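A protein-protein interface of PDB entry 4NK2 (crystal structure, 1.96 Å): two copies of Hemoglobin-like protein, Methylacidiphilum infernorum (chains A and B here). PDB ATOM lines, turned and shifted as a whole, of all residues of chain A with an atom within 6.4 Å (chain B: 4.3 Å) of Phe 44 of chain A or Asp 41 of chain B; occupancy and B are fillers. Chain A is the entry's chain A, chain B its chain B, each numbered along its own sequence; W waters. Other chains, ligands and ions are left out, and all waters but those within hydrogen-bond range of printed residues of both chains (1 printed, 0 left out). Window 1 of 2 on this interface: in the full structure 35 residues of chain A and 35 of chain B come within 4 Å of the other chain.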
ATOM      1  N   PHE A  42      -8.487  27.995  -1.315  1.00  0.00           N
ATOM      2  CA  PHE A  42      -8.254  26.662  -1.884  1.00  0.00           C
ATOM      3  C   PHE A  42      -7.482  25.801  -0.893  1.00  0.00           C
ATOM      4  O   PHE A  42      -6.640  26.309  -0.141  1.00  0.00           O
ATOM      5  CB  PHE A  42      -7.499  26.748  -3.219  1.00  0.00           C
ATOM      6  CG  PHE A  42      -6.086  27.263  -3.094  1.00  0.00           C
ATOM      7  CD1 PHE A  42      -5.006  26.408  -3.277  1.00  0.00           C
ATOM      8  CD2 PHE A  42      -5.835  28.598  -2.795  1.00  0.00           C
ATOM      9  CE1 PHE A  42      -3.699  26.870  -3.167  1.00  0.00           C
ATOM     10  CE2 PHE A  42      -4.532  29.075  -2.685  1.00  0.00           C
ATOM     11  CZ  PHE A  42      -3.459  28.210  -2.870  1.00  0.00           C
ATOM     12  N   VAL A  43      -7.772  24.500  -0.896  1.00  0.00           N
ATOM     13  CA  VAL A  43      -7.109  23.542  -0.011  1.00  0.00           C
ATOM     14  C   VAL A  43      -5.755  23.093  -0.579  1.00  0.00           C
ATOM     15  O   VAL A  43      -5.614  22.920  -1.792  1.00  0.00           O
ATOM     16  CB  VAL A  43      -7.987  22.283   0.187  1.00  0.00           C
ATOM     17  CG1 VAL A  43      -7.366  21.342   1.213  1.00  0.00           C
ATOM     18  CG2 VAL A  43      -9.383  22.677   0.629  1.00  0.00           C
ATOM     19  N   PHE A  44      -4.760  22.915   0.287  1.00  0.00           N
ATOM     20  CA  PHE A  44      -3.547  22.210  -0.111  1.00  0.00           C
ATOM     21  C   PHE A  44      -3.851  20.718  -0.034  1.00  0.00           C
ATOM     22  O   PHE A  44      -3.910  20.154   1.061  1.00  0.00           O
ATOM     23  CB  PHE A  44      -2.381  22.550   0.825  1.00  0.00           C
ATOM     24  CG  PHE A  44      -1.950  23.998   0.771  1.00  0.00           C
ATOM     25  CD1 PHE A  44      -2.322  24.810  -0.292  1.00  0.00           C
ATOM     26  CD2 PHE A  44      -1.157  24.536   1.776  1.00  0.00           C
ATOM     27  CE1 PHE A  44      -1.915  26.150  -0.343  1.00  0.00           C
ATOM     28  CE2 PHE A  44      -0.758  25.866   1.735  1.00  0.00           C
ATOM     29  CZ  PHE A  44      -1.136  26.667   0.669  1.00  0.00           C
ATOM     30  N   PRO A  45      -4.040  20.064  -1.190  1.00  0.00           N
ATOM     31  CA  PRO A  45      -4.402  18.640  -1.120  1.00  0.00           C
ATOM     32  C   PRO A  45      -3.288  17.781  -0.513  1.00  0.00           C
ATOM     33  O   PRO A  45      -2.138  18.222  -0.414  1.00  0.00           O
ATOM     34  CB  PRO A  45      -4.634  18.261  -2.587  1.00  0.00           C
ATOM     35  CG  PRO A  45      -3.894  19.280  -3.379  1.00  0.00           C
ATOM     36  CD  PRO A  45      -3.978  20.552  -2.581  1.00  0.00           C
ATOM     37  N   GLU A  46      -3.615  16.567  -0.114  1.00  0.00           N
ATOM     38  CA  GLU A  46      -2.631  15.644   0.425  1.00  0.00           C
ATOM     39  C   GLU A  46      -1.424  15.502  -0.488  1.00  0.00           C
ATOM     40  O   GLU A  46      -1.571  15.441  -1.689  1.00  0.00           O
ATOM     41  CB  GLU A  46      -3.270  14.276   0.632  1.00  0.00           C
ATOM     42  CG  GLU A  46      -2.403  13.297   1.345  1.00  0.00           C
ATOM     43  CD  GLU A  46      -2.928  11.891   1.271  1.00  0.00           C
ATOM     44  OE1 GLU A  46      -3.850  11.633   0.492  1.00  0.00           O
ATOM     45  OE2 GLU A  46      -2.418  11.034   1.994  1.00  0.00           O
ATOM     46  N   VAL A  47      -0.237  15.435   0.099  1.00  0.00           N
ATOM     47  CA  VAL A  47       1.003  15.209  -0.656  1.00  0.00           C
ATOM     48  C   VAL A  47       1.668  13.880  -0.263  1.00  0.00           C
ATOM     49  O   VAL A  47       2.030  13.670   0.906  1.00  0.00           O
ATOM     50  CB  VAL A  47       2.028  16.323  -0.449  1.00  0.00           C
ATOM     51  CG1 VAL A  47       3.317  15.990  -1.197  1.00  0.00           C
ATOM     52  CG2 VAL A  47       1.478  17.653  -0.929  1.00  0.00           C
ATOM     53  N   ARG A 121       7.380  25.869   1.249  1.00  0.00           N
ATOM     54  CA  ARG A 121       6.452  26.955   0.928  1.00  0.00           C
ATOM     55  C   ARG A 121       7.086  28.250   1.392  1.00  0.00           C
ATOM     56  O   ARG A 121       7.118  29.233   0.649  1.00  0.00           O
ATOM     57  CB  ARG A 121       5.073  26.774   1.589  1.00  0.00           C
ATOM     58  CG  ARG A 121       4.134  27.984   1.389  1.00  0.00           C
ATOM     59  CD  ARG A 121       2.696  27.737   1.874  1.00  0.00           C
ATOM     60  NE  ARG A 121       1.926  28.989   1.857  1.00  0.00           N
ATOM     61  CZ  ARG A 121       1.362  29.500   0.763  1.00  0.00           C
ATOM     62  NH1 ARG A 121       1.465  28.862  -0.405  1.00  0.00           N
ATOM     63  NH2 ARG A 121       0.688  30.643   0.834  1.00  0.00           N
ATOM     64  N   PHE A 125       8.444  31.951  -0.699  1.00  0.00           N
ATOM     65  CA  PHE A 125       7.887  33.301  -0.586  1.00  0.00           C
ATOM     66  C   PHE A 125       8.808  34.317  -1.281  1.00  0.00           C
ATOM     67  O   PHE A 125       8.359  35.389  -1.670  1.00  0.00           O
ATOM     68  CB  PHE A 125       7.672  33.709   0.880  1.00  0.00           C
ATOM     69  CG  PHE A 125       6.498  33.027   1.554  1.00  0.00           C
ATOM     70  CD1 PHE A 125       5.341  32.720   0.848  1.00  0.00           C
ATOM     71  CD2 PHE A 125       6.560  32.707   2.911  1.00  0.00           C
ATOM     72  CE1 PHE A 125       4.263  32.088   1.480  1.00  0.00           C
ATOM     73  CE2 PHE A 125       5.484  32.075   3.554  1.00  0.00           C
ATOM     74  CZ  PHE A 125       4.341  31.768   2.840  1.00  0.00           C
ATOM     75  N   SER A 164       1.266  17.507  -6.659  1.00  0.00           N
ATOM     76  CA  SER A 164       0.546  17.966  -5.476  1.00  0.00           C
ATOM     77  C   SER A 164       1.370  18.930  -4.632  1.00  0.00           C
ATOM     78  O   SER A 164       0.847  19.939  -4.169  1.00  0.00           O
ATOM     79  CB  SER A 164       0.061  16.796  -4.620  1.00  0.00           C
ATOM     80  OG  SER A 164      -0.579  17.299  -3.458  1.00  0.00           O
ATOM     81  N   ILE A 167       1.452  22.620  -5.465  1.00  0.00           N
ATOM     82  CA  ILE A 167       0.319  23.498  -5.148  1.00  0.00           C
ATOM     83  C   ILE A 167       0.627  24.416  -3.953  1.00  0.00           C
ATOM     84  O   ILE A 167       0.173  25.564  -3.909  1.00  0.00           O
ATOM     85  CB  ILE A 167      -0.954  22.696  -4.870  1.00  0.00           C
ATOM     86  CG1 ILE A 167      -1.372  21.930  -6.136  1.00  0.00           C
ATOM     87  CG2 ILE A 167      -2.064  23.621  -4.444  1.00  0.00           C
ATOM     88  CD1 ILE A 167      -2.553  20.991  -5.913  1.00  0.00           C
ATOM     89  N   ARG A 168       1.382  23.903  -2.983  1.00  0.00           N
ATOM     90  CA  ARG A 168       1.698  24.659  -1.771  1.00  0.00           C
ATOM     91  C   ARG A 168       2.750  25.726  -1.980  1.00  0.00           C
ATOM     92  O   ARG A 168       3.037  26.502  -1.064  1.00  0.00           O
ATOM     93  CB  ARG A 168       2.180  23.710  -0.681  1.00  0.00           C
ATOM     94  CG  ARG A 168       1.341  22.470  -0.594  1.00  0.00           C
ATOM     95  CD  ARG A 168       1.601  21.708   0.683  1.00  0.00           C
ATOM     96  NE  ARG A 168       0.577  20.683   0.852  1.00  0.00           N
ATOM     97  CZ  ARG A 168       0.227  20.161   2.019  1.00  0.00           C
ATOM     98  NH1 ARG A 168       0.822  20.569   3.132  1.00  0.00           N
ATOM     99  NH2 ARG A 168      -0.724  19.241   2.066  1.00  0.00           N
ATOM    100  N   MET A 169       3.349  25.775  -3.165  1.00  0.00           N
ATOM    101  CA  MET A 169       4.307  26.855  -3.433  1.00  0.00           C
ATOM    102  C   MET A 169       3.600  28.115  -3.941  1.00  0.00           C
ATOM    103  O   MET A 169       4.185  29.204  -3.950  1.00  0.00           O
ATOM    104  CB  MET A 169       5.343  26.402  -4.451  1.00  0.00           C
ATOM    105  CG  MET A 169       6.018  25.075  -4.077  1.00  0.00           C
ATOM    106  SD  MET A 169       6.675  25.150  -2.397  1.00  0.00           S
ATOM    107  CE  MET A 169       6.339  23.437  -2.013  1.00  0.00           C
ATOM    108  N   ILE A 170       2.349  27.967  -4.380  1.00  0.00           N
ATOM    109  CA  ILE A 170       1.640  29.089  -5.005  1.00  0.00           C
ATOM    110  C   ILE A 170       1.395  30.168  -3.951  1.00  0.00           C
ATOM    111  O   ILE A 170       0.768  29.907  -2.913  1.00  0.00           O
ATOM    112  CB  ILE A 170       0.274  28.677  -5.598  1.00  0.00           C
ATOM    113  CG1 ILE A 170       0.464  27.713  -6.780  1.00  0.00           C
ATOM    114  CG2 ILE A 170      -0.497  29.924  -6.044  1.00  0.00           C
ATOM    115  CD1 ILE A 170      -0.849  27.159  -7.328  1.00  0.00           C
ATOM    116  N   ALA B  38      -3.953  16.939   3.732  1.00  0.00           N
ATOM    117  CA  ALA B  38      -4.467  18.172   3.156  1.00  0.00           C
ATOM    118  C   ALA B  38      -4.516  19.231   4.262  1.00  0.00           C
ATOM    119  O   ALA B  38      -4.715  18.897   5.437  1.00  0.00           O
ATOM    120  CB  ALA B  38      -5.855  17.941   2.554  1.00  0.00           C
ATOM    121  N   ARG B  39      -4.319  20.491   3.899  1.00  0.00           N
ATOM    122  CA  ARG B  39      -4.376  21.584   4.862  1.00  0.00           C
ATOM    123  C   ARG B  39      -4.828  22.885   4.225  1.00  0.00           C
ATOM    124  O   ARG B  39      -4.866  23.006   3.018  1.00  0.00           O
ATOM    125  CB  ARG B  39      -3.032  21.769   5.551  1.00  0.00           C
ATOM    126  CG  ARG B  39      -1.971  22.352   4.673  1.00  0.00           C
ATOM    127  CD  ARG B  39      -0.720  22.681   5.440  1.00  0.00           C
ATOM    128  NE  ARG B  39      -0.912  23.874   6.239  1.00  0.00           N
ATOM    129  CZ  ARG B  39      -0.326  25.043   6.013  1.00  0.00           C
ATOM    130  NH1 ARG B  39       0.520  25.197   5.012  1.00  0.00           N
ATOM    131  NH2 ARG B  39      -0.589  26.061   6.808  1.00  0.00           N
ATOM    132  N   ILE B  40      -5.193  23.859   5.044  1.00  0.00           N
ATOM    133  CA  ILE B  40      -5.574  25.158   4.510  1.00  0.00           C
ATOM    134  C   ILE B  40      -4.538  26.185   4.930  1.00  0.00           C
ATOM    135  O   ILE B  40      -3.924  26.067   5.993  1.00  0.00           O
ATOM    136  CB  ILE B  40      -6.965  25.596   4.997  1.00  0.00           C
ATOM    137  CG1 ILE B  40      -6.925  25.893   6.494  1.00  0.00           C
ATOM    138  CG2 ILE B  40      -8.001  24.520   4.694  1.00  0.00           C
ATOM    139  CD1 ILE B  40      -8.239  26.391   7.046  1.00  0.00           C
ATOM    140  N   ASP B  41      -4.335  27.188   4.089  1.00  0.00           N
ATOM    141  CA  ASP B  41      -3.379  28.232   4.395  1.00  0.00           C
ATOM    142  C   ASP B  41      -3.956  29.145   5.477  1.00  0.00           C
ATOM    143  O   ASP B  41      -3.463  29.177   6.615  1.00  0.00           O
ATOM    144  CB  ASP B  41      -3.054  29.020   3.128  1.00  0.00           C
ATOM    145  CG  ASP B  41      -2.109  30.175   3.384  1.00  0.00           C
ATOM    146  OD1 ASP B  41      -1.460  30.198   4.464  1.00  0.00           O
ATOM    147  OD2 ASP B  41      -1.997  31.054   2.494  1.00  0.00           O
ATOM    148  N   PHE B  42      -4.999  29.888   5.119  1.00  0.00           N
ATOM    149  CA  PHE B  42      -5.721  30.704   6.097  1.00  0.00           C
ATOM    150  C   PHE B  42      -7.213  30.797   5.758  1.00  0.00           C
ATOM    151  O   PHE B  42      -7.594  30.806   4.588  1.00  0.00           O
ATOM    152  CB  PHE B  42      -5.090  32.106   6.239  1.00  0.00           C
ATOM    153  CG  PHE B  42      -5.218  32.968   5.012  1.00  0.00           C
ATOM    154  CD1 PHE B  42      -4.428  32.732   3.895  1.00  0.00           C
ATOM    155  CD2 PHE B  42      -6.117  34.031   4.983  1.00  0.00           C
ATOM    156  CE1 PHE B  42      -4.540  33.531   2.760  1.00  0.00           C
ATOM    157  CE2 PHE B  42      -6.232  34.837   3.858  1.00  0.00           C
ATOM    158  CZ  PHE B  42      -5.437  34.587   2.743  1.00  0.00           C
ATOM    159  N   ARG B 173       0.793  36.039  -0.578  1.00  0.00           N
ATOM    160  CA  ARG B 173       1.173  35.567   0.756  1.00  0.00           C
ATOM    161  C   ARG B 173       2.685  35.658   0.945  1.00  0.00           C
ATOM    162  O   ARG B 173       3.438  35.366   0.009  1.00  0.00           O
ATOM    163  CB  ARG B 173       0.686  34.127   0.955  1.00  0.00           C
ATOM    164  CG  ARG B 173      -0.815  34.048   1.134  1.00  0.00           C
ATOM    165  CD  ARG B 173      -1.201  34.609   2.490  1.00  0.00           C
ATOM    166  NE  ARG B 173      -1.231  33.570   3.528  1.00  0.00           N
ATOM    167  CZ  ARG B 173      -1.041  33.801   4.823  1.00  0.00           C
ATOM    168  NH1 ARG B 173      -0.769  35.035   5.248  1.00  0.00           N
ATOM    169  NH2 ARG B 173      -1.108  32.799   5.685  1.00  0.00           N
HETATM  170  O   HOH W   1       1.120  30.960   3.782  1.00  0.00           O
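N of Phe 44 of chain A sits at hydrogen-bond distance from O of Arg 39 of chain B (2.7 Å). The guanidinium group (NH2) of Arg 121 of chain A is in salt-bridge range of the side-chain carboxylate (OD2) of Asp 41 of chain B (3.2 Å).
The guanidinium group of Arg 168 of chain A sits at hydrogen-bond distance from the backbone carbonyl oxygen of Phe 44 of chain A (3.5 Å). The backbone carbonyl oxygen of Pro 45 of chain A lies within hydrogen-bond range of the guanidinium group of Arg 168 of chain A, 3.0 Å away. O of Glu 46 of chain A lies within hydrogen-bond range of OG of Ser 164 of chain A (2.8 Å). The guanidinium group of Arg 121 of chain A lies within hydrogen-bond range of the backbone carbonyl oxygen of Arg 168 of chain A (2.9 Å). SD of Met 169 of chain A lies within hydrogen-bond range of N of Arg 121 of chain A, at 3.8 Å. The guanidinium group (NE) of Arg 173 of chain B lies within salt-bridge range of the side-chain carboxylate (OD2) of Asp 41 of chain B.
Among the printed residues, pairs that only touch across the chains: Phe 44 of chain A with Ala 38 of chain B, Phe 125 of chain A with Arg 173 of chain B, Arg 121 of chain A with Arg 173 of chain B, Arg 168 of chain A with Arg 39 of chain B, Val 43 of chain A with Arg 39 of chain B, Glu 46 of chain A with Ala 38 of chain B, Pro 45 of chain A with Ala 38 of chain B, Phe 44 of chain A with Asp 41 of chain B and Val 43 of chain A with Ala 38 of chain B.
Phe 42 of chain A touches none of the printed residues of chain B. Of the printed residues of chain B, Val 43 of chain A touches Ala 38 (3.96 Å) and Arg 39 (3.5 Å). Of chain B, only Ala 38, Arg 39 and Asp 41 come within 4 Å of Phe 44 of chain A. Ser 164 of chain A touches none of the printed residues of chain B. Asp 41 of chain B touches two residues of chain A. Printed residues of chain A within 4 Å of Arg 173 of chain B: Arg 121 and Phe 125. The nearest printed residue of chain B that does not touch Phe 44 of chain A is Ile 40 of chain B (4.9 Å). The nearest residue of chain A that does not touch Asp 41 of chain B is Phe 42 of chain A (4.9 Å). The nearest printed residue of chain B that does not touch Arg 168 of chain A is Ala 38 of chain B (4.04 Å).
Hydrophobic or aromatic side chains of chain A that line the printed part of chain B: Val 43, Phe 44 and Phe 125. Of the 6 printed residues of chain B, 4 touch a printed residue of chain A. Hydrophobic or aromatic side chains of chain B within 4 Å of the printed part of chain A: Ala 38. Among the printed residues, 11 pairs touch across the chains.
Position printed for both chains: 42. Of the 11 pairs that touch across the chains among the printed residues, none has its exchanged pair printed and touching as well.
Water W1 lies within hydrogen-bond range of OD1 of Asp 41 of chain B (2.8 Å), NE of Arg 121 of chain A (2.9 Å) and NH2 of Arg 173 of chain B (3.5 Å).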
